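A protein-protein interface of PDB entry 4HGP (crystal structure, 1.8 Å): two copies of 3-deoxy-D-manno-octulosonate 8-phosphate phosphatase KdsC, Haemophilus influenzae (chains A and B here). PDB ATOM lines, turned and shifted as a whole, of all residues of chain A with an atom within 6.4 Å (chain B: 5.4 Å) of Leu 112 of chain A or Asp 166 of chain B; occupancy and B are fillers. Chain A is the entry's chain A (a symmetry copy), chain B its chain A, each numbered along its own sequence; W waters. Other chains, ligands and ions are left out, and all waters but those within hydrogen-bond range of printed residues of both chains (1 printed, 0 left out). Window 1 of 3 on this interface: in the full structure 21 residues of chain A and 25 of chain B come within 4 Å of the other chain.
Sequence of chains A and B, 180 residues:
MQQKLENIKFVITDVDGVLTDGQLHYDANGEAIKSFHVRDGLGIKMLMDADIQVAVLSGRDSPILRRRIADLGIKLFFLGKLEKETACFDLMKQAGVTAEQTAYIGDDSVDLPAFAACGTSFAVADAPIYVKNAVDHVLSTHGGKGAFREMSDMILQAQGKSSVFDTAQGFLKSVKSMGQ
Of the 8 printed residues of chain B, 4 touch a printed residue of chain A.
Printed residues of chain B that touch a printed residue of chain A: Phe 165, Asp 166, Thr 167 and Ala 168.
Of the 14 printed residues of chain A, 4 touch a printed residue of chain B.
Printed residues of chain A that touch a printed residue of chain B: Ser 109, Leu 112, Pro 113 and Tyr 130.
Among the printed residues, no Asp or Glu carboxylate lies within 4 Å of a Lys or Arg side-chain nitrogen of the other chain.
Leu 112 of chain A touches Phe 165 of chain B (CD1 to O, 3.5 Å).
Leu 112 of chain A touches Asp 166 of chain B.
C of Thr 167 of chain B touches CD1 of Leu 112 of chain A, at 3.7 Å.
Ala 168 of chain B touches Leu 112 of chain A (N to CD1, 3.8 Å).
N of Pro 113 of chain A touches CB of Ala 168 of chain B, 3.9 Å away.
O of Phe 165 of chain B touches CD1 of Tyr 130 of chain A, at 3.2 Å.
CB of Tyr 130 of chain A touches CB of Asp 166 of chain B, at 3.7 Å.
No position is printed for both chains.
The backbone carbonyl oxygen (O) of Ser 163 of chain B is in hydrogen-bond range of the side-chain hydroxyl (OG1) of Thr 167 of chain B (2.9 Å).
The side-chain carboxylate (OD2) of Asp 166 of chain B is in hydrogen-bond range of the side-chain hydroxyl (OG) of Ser 162 of chain B.
Water W1 lies within hydrogen-bond range of the backbone carbonyl oxygen (O) of Asp 166 of chain B (2.5 Å) and the backbone carbonyl oxygen (O) of Tyr 130 of chain A (2.7 Å).
The backbone carbonyl oxygen of Phe 165 of chain B is in hydrogen-bond range of the side-chain hydroxyl of Ser 109 of chain A.
Of chain B, only Phe 165, Asp 166, Thr 167 and Ala 168 come within 4 Å of Leu 112 of chain A.
Of the printed residues of chain B, Tyr 130 of chain A touches Phe 165 and Asp 166.
Val 164 of chain B touches none of the printed residues of chain A.
Of the printed residues of chain A, Phe 165 of chain B touches Ser 109, Leu 112 and Tyr 130.
Of chain A, only Leu 112 and Tyr 130 come within 4 Å of Asp 166 of chain B.
Of the printed residues of chain A, Thr 167 of chain B touches Leu 112 (3.7 Å).
The nearest printed residue of chain B that does not touch Leu 112 of chain A is Ser 163 of chain B (6.0 Å).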
ATOM      1  N   TYR A 104     -22.241 -20.086 -18.691  1.00  0.00           N
ATOM      2  CA  TYR A 104     -21.070 -20.729 -19.288  1.00  0.00           C
ATOM      3  C   TYR A 104     -20.162 -21.245 -18.189  1.00  0.00           C
ATOM      4  O   TYR A 104     -19.979 -20.587 -17.174  1.00  0.00           O
ATOM      5  CB  TYR A 104     -20.282 -19.753 -20.177  1.00  0.00           C
ATOM      6  CG  TYR A 104     -19.121 -20.390 -20.929  1.00  0.00           C
ATOM      7  CD1 TYR A 104     -19.303 -20.915 -22.202  1.00  0.00           C
ATOM      8  CD2 TYR A 104     -17.846 -20.471 -20.364  1.00  0.00           C
ATOM      9  CE1 TYR A 104     -18.254 -21.499 -22.898  1.00  0.00           C
ATOM     10  CE2 TYR A 104     -16.793 -21.061 -21.052  1.00  0.00           C
ATOM     11  CZ  TYR A 104     -17.004 -21.571 -22.324  1.00  0.00           C
ATOM     12  OH  TYR A 104     -15.976 -22.161 -23.033  1.00  0.00           O
ATOM     13  N   ASP A 108     -10.057 -22.199 -18.229  1.00  0.00           N
ATOM     14  CA  ASP A 108      -8.786 -21.635 -18.666  1.00  0.00           C
ATOM     15  C   ASP A 108      -8.975 -20.345 -19.464  1.00  0.00           C
ATOM     16  O   ASP A 108     -10.100 -19.937 -19.748  1.00  0.00           O
ATOM     17  CB  ASP A 108      -7.979 -22.679 -19.458  1.00  0.00           C
ATOM     18  CG  ASP A 108      -6.478 -22.389 -19.479  1.00  0.00           C
ATOM     19  OD1 ASP A 108      -6.003 -21.543 -18.690  1.00  0.00           O
ATOM     20  OD2 ASP A 108      -5.768 -23.032 -20.285  1.00  0.00           O
ATOM     21  N   SER A 109      -7.858 -19.722 -19.820  1.00  0.00           N
ATOM     22  CA  SER A 109      -7.833 -18.433 -20.505  1.00  0.00           C
ATOM     23  C   SER A 109      -8.733 -18.362 -21.742  1.00  0.00           C
ATOM     24  O   SER A 109      -9.332 -17.318 -22.010  1.00  0.00           O
ATOM     25  CB  SER A 109      -6.394 -18.085 -20.876  1.00  0.00           C
ATOM     26  OG  SER A 109      -5.575 -18.002 -19.724  1.00  0.00           O
ATOM     27  N   VAL A 110      -8.834 -19.468 -22.480  1.00  0.00           N
ATOM     28  CA  VAL A 110      -9.606 -19.528 -23.724  1.00  0.00           C
ATOM     29  C   VAL A 110     -11.092 -19.281 -23.457  1.00  0.00           C
ATOM     30  O   VAL A 110     -11.858 -18.902 -24.350  1.00  0.00           O
ATOM     31  CB  VAL A 110      -9.413 -20.894 -24.434  1.00  0.00           C
ATOM     32  CG1 VAL A 110     -10.069 -22.017 -23.638  1.00  0.00           C
ATOM     33  CG2 VAL A 110      -9.957 -20.863 -25.860  1.00  0.00           C
ATOM     34  N   ASP A 111     -11.479 -19.477 -22.204  1.00  0.00           N
ATOM     35  CA  ASP A 111     -12.859 -19.320 -21.782  1.00  0.00           C
ATOM     36  C   ASP A 111     -13.172 -17.892 -21.363  1.00  0.00           C
ATOM     37  O   ASP A 111     -14.335 -17.532 -21.222  1.00  0.00           O
ATOM     38  CB  ASP A 111     -13.143 -20.265 -20.621  1.00  0.00           C
ATOM     39  CG  ASP A 111     -12.984 -21.723 -21.009  1.00  0.00           C
ATOM     40  OD1 ASP A 111     -13.617 -22.143 -21.995  1.00  0.00           O
ATOM     41  OD2 ASP A 111     -12.232 -22.448 -20.325  1.00  0.00           O
ATOM     42  N   LEU A 112     -12.129 -17.090 -21.150  1.00  0.00           N
ATOM     43  CA  LEU A 112     -12.289 -15.694 -20.743  1.00  0.00           C
ATOM     44  C   LEU A 112     -13.213 -14.868 -21.659  1.00  0.00           C
ATOM     45  O   LEU A 112     -14.005 -14.079 -21.161  1.00  0.00           O
ATOM     46  CB  LEU A 112     -10.933 -14.998 -20.581  1.00  0.00           C
ATOM     47  CG  LEU A 112     -10.037 -15.379 -19.399  1.00  0.00           C
ATOM     48  CD1 LEU A 112      -8.734 -14.595 -19.477  1.00  0.00           C
ATOM     49  CD2 LEU A 112     -10.728 -15.160 -18.060  1.00  0.00           C
ATOM     50  N   PRO A 113     -13.124 -15.043 -22.995  1.00  0.00           N
ATOM     51  CA  PRO A 113     -14.115 -14.323 -23.809  1.00  0.00           C
ATOM     52  C   PRO A 113     -15.546 -14.882 -23.664  1.00  0.00           C
ATOM     53  O   PRO A 113     -16.511 -14.138 -23.808  1.00  0.00           O
ATOM     54  CB  PRO A 113     -13.598 -14.516 -25.240  1.00  0.00           C
ATOM     55  CG  PRO A 113     -12.175 -14.871 -25.087  1.00  0.00           C
ATOM     56  CD  PRO A 113     -12.092 -15.665 -23.840  1.00  0.00           C
ATOM     57  N   ALA A 114     -15.676 -16.173 -23.375  1.00  0.00           N
ATOM     58  CA  ALA A 114     -16.992 -16.773 -23.164  1.00  0.00           C
ATOM     59  C   ALA A 114     -17.654 -16.230 -21.899  1.00  0.00           C
ATOM     60  O   ALA A 114     -18.872 -16.044 -21.855  1.00  0.00           O
ATOM     61  CB  ALA A 114     -16.887 -18.276 -23.103  1.00  0.00           C
ATOM     62  N   PHE A 115     -16.843 -15.985 -20.872  1.00  0.00           N
ATOM     63  CA  PHE A 115     -17.326 -15.426 -19.624  1.00  0.00           C
ATOM     64  C   PHE A 115     -17.897 -14.041 -19.871  1.00  0.00           C
ATOM     65  O   PHE A 115     -18.874 -13.642 -19.242  1.00  0.00           O
ATOM     66  CB  PHE A 115     -16.194 -15.344 -18.599  1.00  0.00           C
ATOM     67  CG  PHE A 115     -15.650 -16.684 -18.177  1.00  0.00           C
ATOM     68  CD1 PHE A 115     -16.470 -17.804 -18.138  1.00  0.00           C
ATOM     69  CD2 PHE A 115     -14.317 -16.819 -17.816  1.00  0.00           C
ATOM     70  CE1 PHE A 115     -15.965 -19.040 -17.746  1.00  0.00           C
ATOM     71  CE2 PHE A 115     -13.805 -18.044 -17.426  1.00  0.00           C
ATOM     72  CZ  PHE A 115     -14.632 -19.157 -17.385  1.00  0.00           C
ATOM     73  N   ALA A 116     -17.283 -13.315 -20.802  1.00  0.00           N
ATOM     74  CA  ALA A 116     -17.700 -11.956 -21.125  1.00  0.00           C
ATOM     75  C   ALA A 116     -18.989 -11.938 -21.951  1.00  0.00           C
ATOM     76  O   ALA A 116     -19.791 -11.009 -21.843  1.00  0.00           O
ATOM     77  CB  ALA A 116     -16.586 -11.234 -21.862  1.00  0.00           C
ATOM     78  N   ALA A 117     -19.186 -12.966 -22.770  1.00  0.00           N
ATOM     79  CA  ALA A 117     -20.364 -13.041 -23.623  1.00  0.00           C
ATOM     80  C   ALA A 117     -21.623 -13.459 -22.861  1.00  0.00           C
ATOM     81  O   ALA A 117     -22.705 -12.947 -23.127  1.00  0.00           O
ATOM     82  CB  ALA A 117     -20.116 -13.971 -24.805  1.00  0.00           C
ATOM     83  N   TYR A 130      -6.702 -16.313 -12.297  1.00  0.00           N
ATOM     84  CA  TYR A 130      -7.166 -15.327 -13.265  1.00  0.00           C
ATOM     85  C   TYR A 130      -8.452 -15.744 -13.972  1.00  0.00           C
ATOM     86  O   TYR A 130      -9.098 -14.924 -14.612  1.00  0.00           O
ATOM     87  CB  TYR A 130      -6.074 -15.000 -14.277  1.00  0.00           C
ATOM     88  CG  TYR A 130      -5.278 -16.189 -14.754  1.00  0.00           C
ATOM     89  CD1 TYR A 130      -5.670 -16.910 -15.879  1.00  0.00           C
ATOM     90  CD2 TYR A 130      -4.117 -16.581 -14.097  1.00  0.00           C
ATOM     91  CE1 TYR A 130      -4.936 -17.991 -16.333  1.00  0.00           C
ATOM     92  CE2 TYR A 130      -3.378 -17.664 -14.538  1.00  0.00           C
ATOM     93  CZ  TYR A 130      -3.793 -18.366 -15.659  1.00  0.00           C
ATOM     94  OH  TYR A 130      -3.054 -19.441 -16.108  1.00  0.00           O
ATOM     95  N   VAL A 131      -8.813 -17.020 -13.850  1.00  0.00           N
ATOM     96  CA  VAL A 131     -10.085 -17.512 -14.362  1.00  0.00           C
ATOM     97  C   VAL A 131     -11.158 -17.388 -13.287  1.00  0.00           C
ATOM     98  O   VAL A 131     -12.275 -16.948 -13.570  1.00  0.00           O
ATOM     99  CB  VAL A 131      -9.966 -18.960 -14.865  1.00  0.00           C
ATOM    100  CG1 VAL A 131     -11.335 -19.584 -15.040  1.00  0.00           C
ATOM    101  CG2 VAL A 131      -9.186 -18.980 -16.174  1.00  0.00           C
ATOM    102  N   ALA A 134     -12.682 -14.031 -12.923  1.00  0.00           N
ATOM    103  CA  ALA A 134     -13.474 -13.548 -14.041  1.00  0.00           C
ATOM    104  C   ALA A 134     -14.905 -14.098 -14.053  1.00  0.00           C
ATOM    105  O   ALA A 134     -15.731 -13.670 -14.861  1.00  0.00           O
ATOM    106  CB  ALA A 134     -12.765 -13.873 -15.345  1.00  0.00           C
ATOM    107  N   GLN B 157       4.682 -13.765 -16.644  1.00  0.00           N
ATOM    108  CA  GLN B 157       4.378 -12.653 -15.749  1.00  0.00           C
ATOM    109  C   GLN B 157       5.625 -11.886 -15.300  1.00  0.00           C
ATOM    110  O   GLN B 157       5.591 -10.668 -15.167  1.00  0.00           O
ATOM    111  CB  GLN B 157       3.592 -13.131 -14.537  1.00  0.00           C
ATOM    112  CG  GLN B 157       3.236 -12.000 -13.599  1.00  0.00           C
ATOM    113  CD  GLN B 157       1.999 -12.284 -12.794  1.00  0.00           C
ATOM    114  OE1 GLN B 157       0.980 -12.696 -13.340  1.00  0.00           O
ATOM    115  NE2 GLN B 157       2.079 -12.072 -11.486  1.00  0.00           N
ATOM    116  N   SER B 162       1.868 -11.284 -19.069  1.00  0.00           N
ATOM    117  CA  SER B 162       0.748 -12.048 -18.526  1.00  0.00           C
ATOM    118  C   SER B 162      -0.608 -11.809 -19.198  1.00  0.00           C
ATOM    119  O   SER B 162      -1.531 -12.602 -19.007  1.00  0.00           O
ATOM    120  CB  SER B 162       0.633 -11.837 -17.017  1.00  0.00           C
ATOM    121  OG  SER B 162       0.189 -10.531 -16.706  1.00  0.00           O
ATOM    122  N   SER B 163      -0.743 -10.734 -19.972  1.00  0.00           N
ATOM    123  CA  SER B 163      -2.033 -10.427 -20.611  1.00  0.00           C
ATOM    124  C   SER B 163      -2.587 -11.567 -21.477  1.00  0.00           C
ATOM    125  O   SER B 163      -3.806 -11.780 -21.538  1.00  0.00           O
ATOM    126  CB  SER B 163      -1.948  -9.137 -21.428  1.00  0.00           C
ATOM    127  OG  SER B 163      -0.857  -9.185 -22.325  1.00  0.00           O
ATOM    128  N   VAL B 164      -1.687 -12.306 -22.125  1.00  0.00           N
ATOM    129  CA  VAL B 164      -2.070 -13.423 -22.987  1.00  0.00           C
ATOM    130  C   VAL B 164      -2.894 -14.465 -22.229  1.00  0.00           C
ATOM    131  O   VAL B 164      -3.692 -15.190 -22.831  1.00  0.00           O
ATOM    132  CB  VAL B 164      -0.831 -14.087 -23.658  1.00  0.00           C
ATOM    133  CG1 VAL B 164       0.029 -14.778 -22.624  1.00  0.00           C
ATOM    134  CG2 VAL B 164      -1.252 -15.069 -24.755  1.00  0.00           C
ATOM    135  N   PHE B 165      -2.731 -14.524 -20.909  1.00  0.00           N
ATOM    136  CA  PHE B 165      -3.488 -15.490 -20.116  1.00  0.00           C
ATOM    137  C   PHE B 165      -4.480 -14.899 -19.109  1.00  0.00           C
ATOM    138  O   PHE B 165      -5.469 -15.539 -18.761  1.00  0.00           O
ATOM    139  CB  PHE B 165      -2.579 -16.564 -19.479  1.00  0.00           C
ATOM    140  CG  PHE B 165      -1.704 -16.074 -18.336  1.00  0.00           C
ATOM    141  CD1 PHE B 165      -2.239 -15.800 -17.087  1.00  0.00           C
ATOM    142  CD2 PHE B 165      -0.339 -15.955 -18.504  1.00  0.00           C
ATOM    143  CE1 PHE B 165      -1.434 -15.376 -16.047  1.00  0.00           C
ATOM    144  CE2 PHE B 165       0.471 -15.540 -17.463  1.00  0.00           C
ATOM    145  CZ  PHE B 165      -0.079 -15.248 -16.239  1.00  0.00           C
ATOM    146  N   ASP B 166      -4.235 -13.681 -18.642  1.00  0.00           N
ATOM    147  CA  ASP B 166      -5.132 -13.124 -17.631  1.00  0.00           C
ATOM    148  C   ASP B 166      -6.173 -12.113 -18.144  1.00  0.00           C
ATOM    149  O   ASP B 166      -6.960 -11.589 -17.360  1.00  0.00           O
ATOM    150  CB  ASP B 166      -4.351 -12.575 -16.428  1.00  0.00           C
ATOM    151  CG  ASP B 166      -3.491 -11.380 -16.773  1.00  0.00           C
ATOM    152  OD1 ASP B 166      -3.708 -10.756 -17.828  1.00  0.00           O
ATOM    153  OD2 ASP B 166      -2.600 -11.043 -15.972  1.00  0.00           O
ATOM    154  N   THR B 167      -6.176 -11.838 -19.447  1.00  0.00           N
ATOM    155  CA  THR B 167      -7.205 -10.972 -20.035  1.00  0.00           C
ATOM    156  C   THR B 167      -7.776 -11.556 -21.326  1.00  0.00           C
ATOM    157  O   THR B 167      -7.045 -12.119 -22.136  1.00  0.00           O
ATOM    158  CB  THR B 167      -6.689  -9.546 -20.329  1.00  0.00           C
ATOM    159  OG1 THR B 167      -5.745  -9.580 -21.410  1.00  0.00           O
ATOM    160  CG2 THR B 167      -6.049  -8.928 -19.103  1.00  0.00           C
ATOM    161  N   ALA B 168      -9.084 -11.422 -21.517  1.00  0.00           N
ATOM    162  CA  ALA B 168      -9.720 -11.894 -22.742  1.00  0.00           C
ATOM    163  C   ALA B 168      -9.090 -11.245 -23.964  1.00  0.00           C
ATOM    164  O   ALA B 168      -8.852 -11.904 -24.973  1.00  0.00           O
ATOM    165  CB  ALA B 168     -11.222 -11.621 -22.708  1.00  0.00           C
HETATM  166  O   HOH W   1      -8.283 -12.494 -15.492  1.00  0.00           O
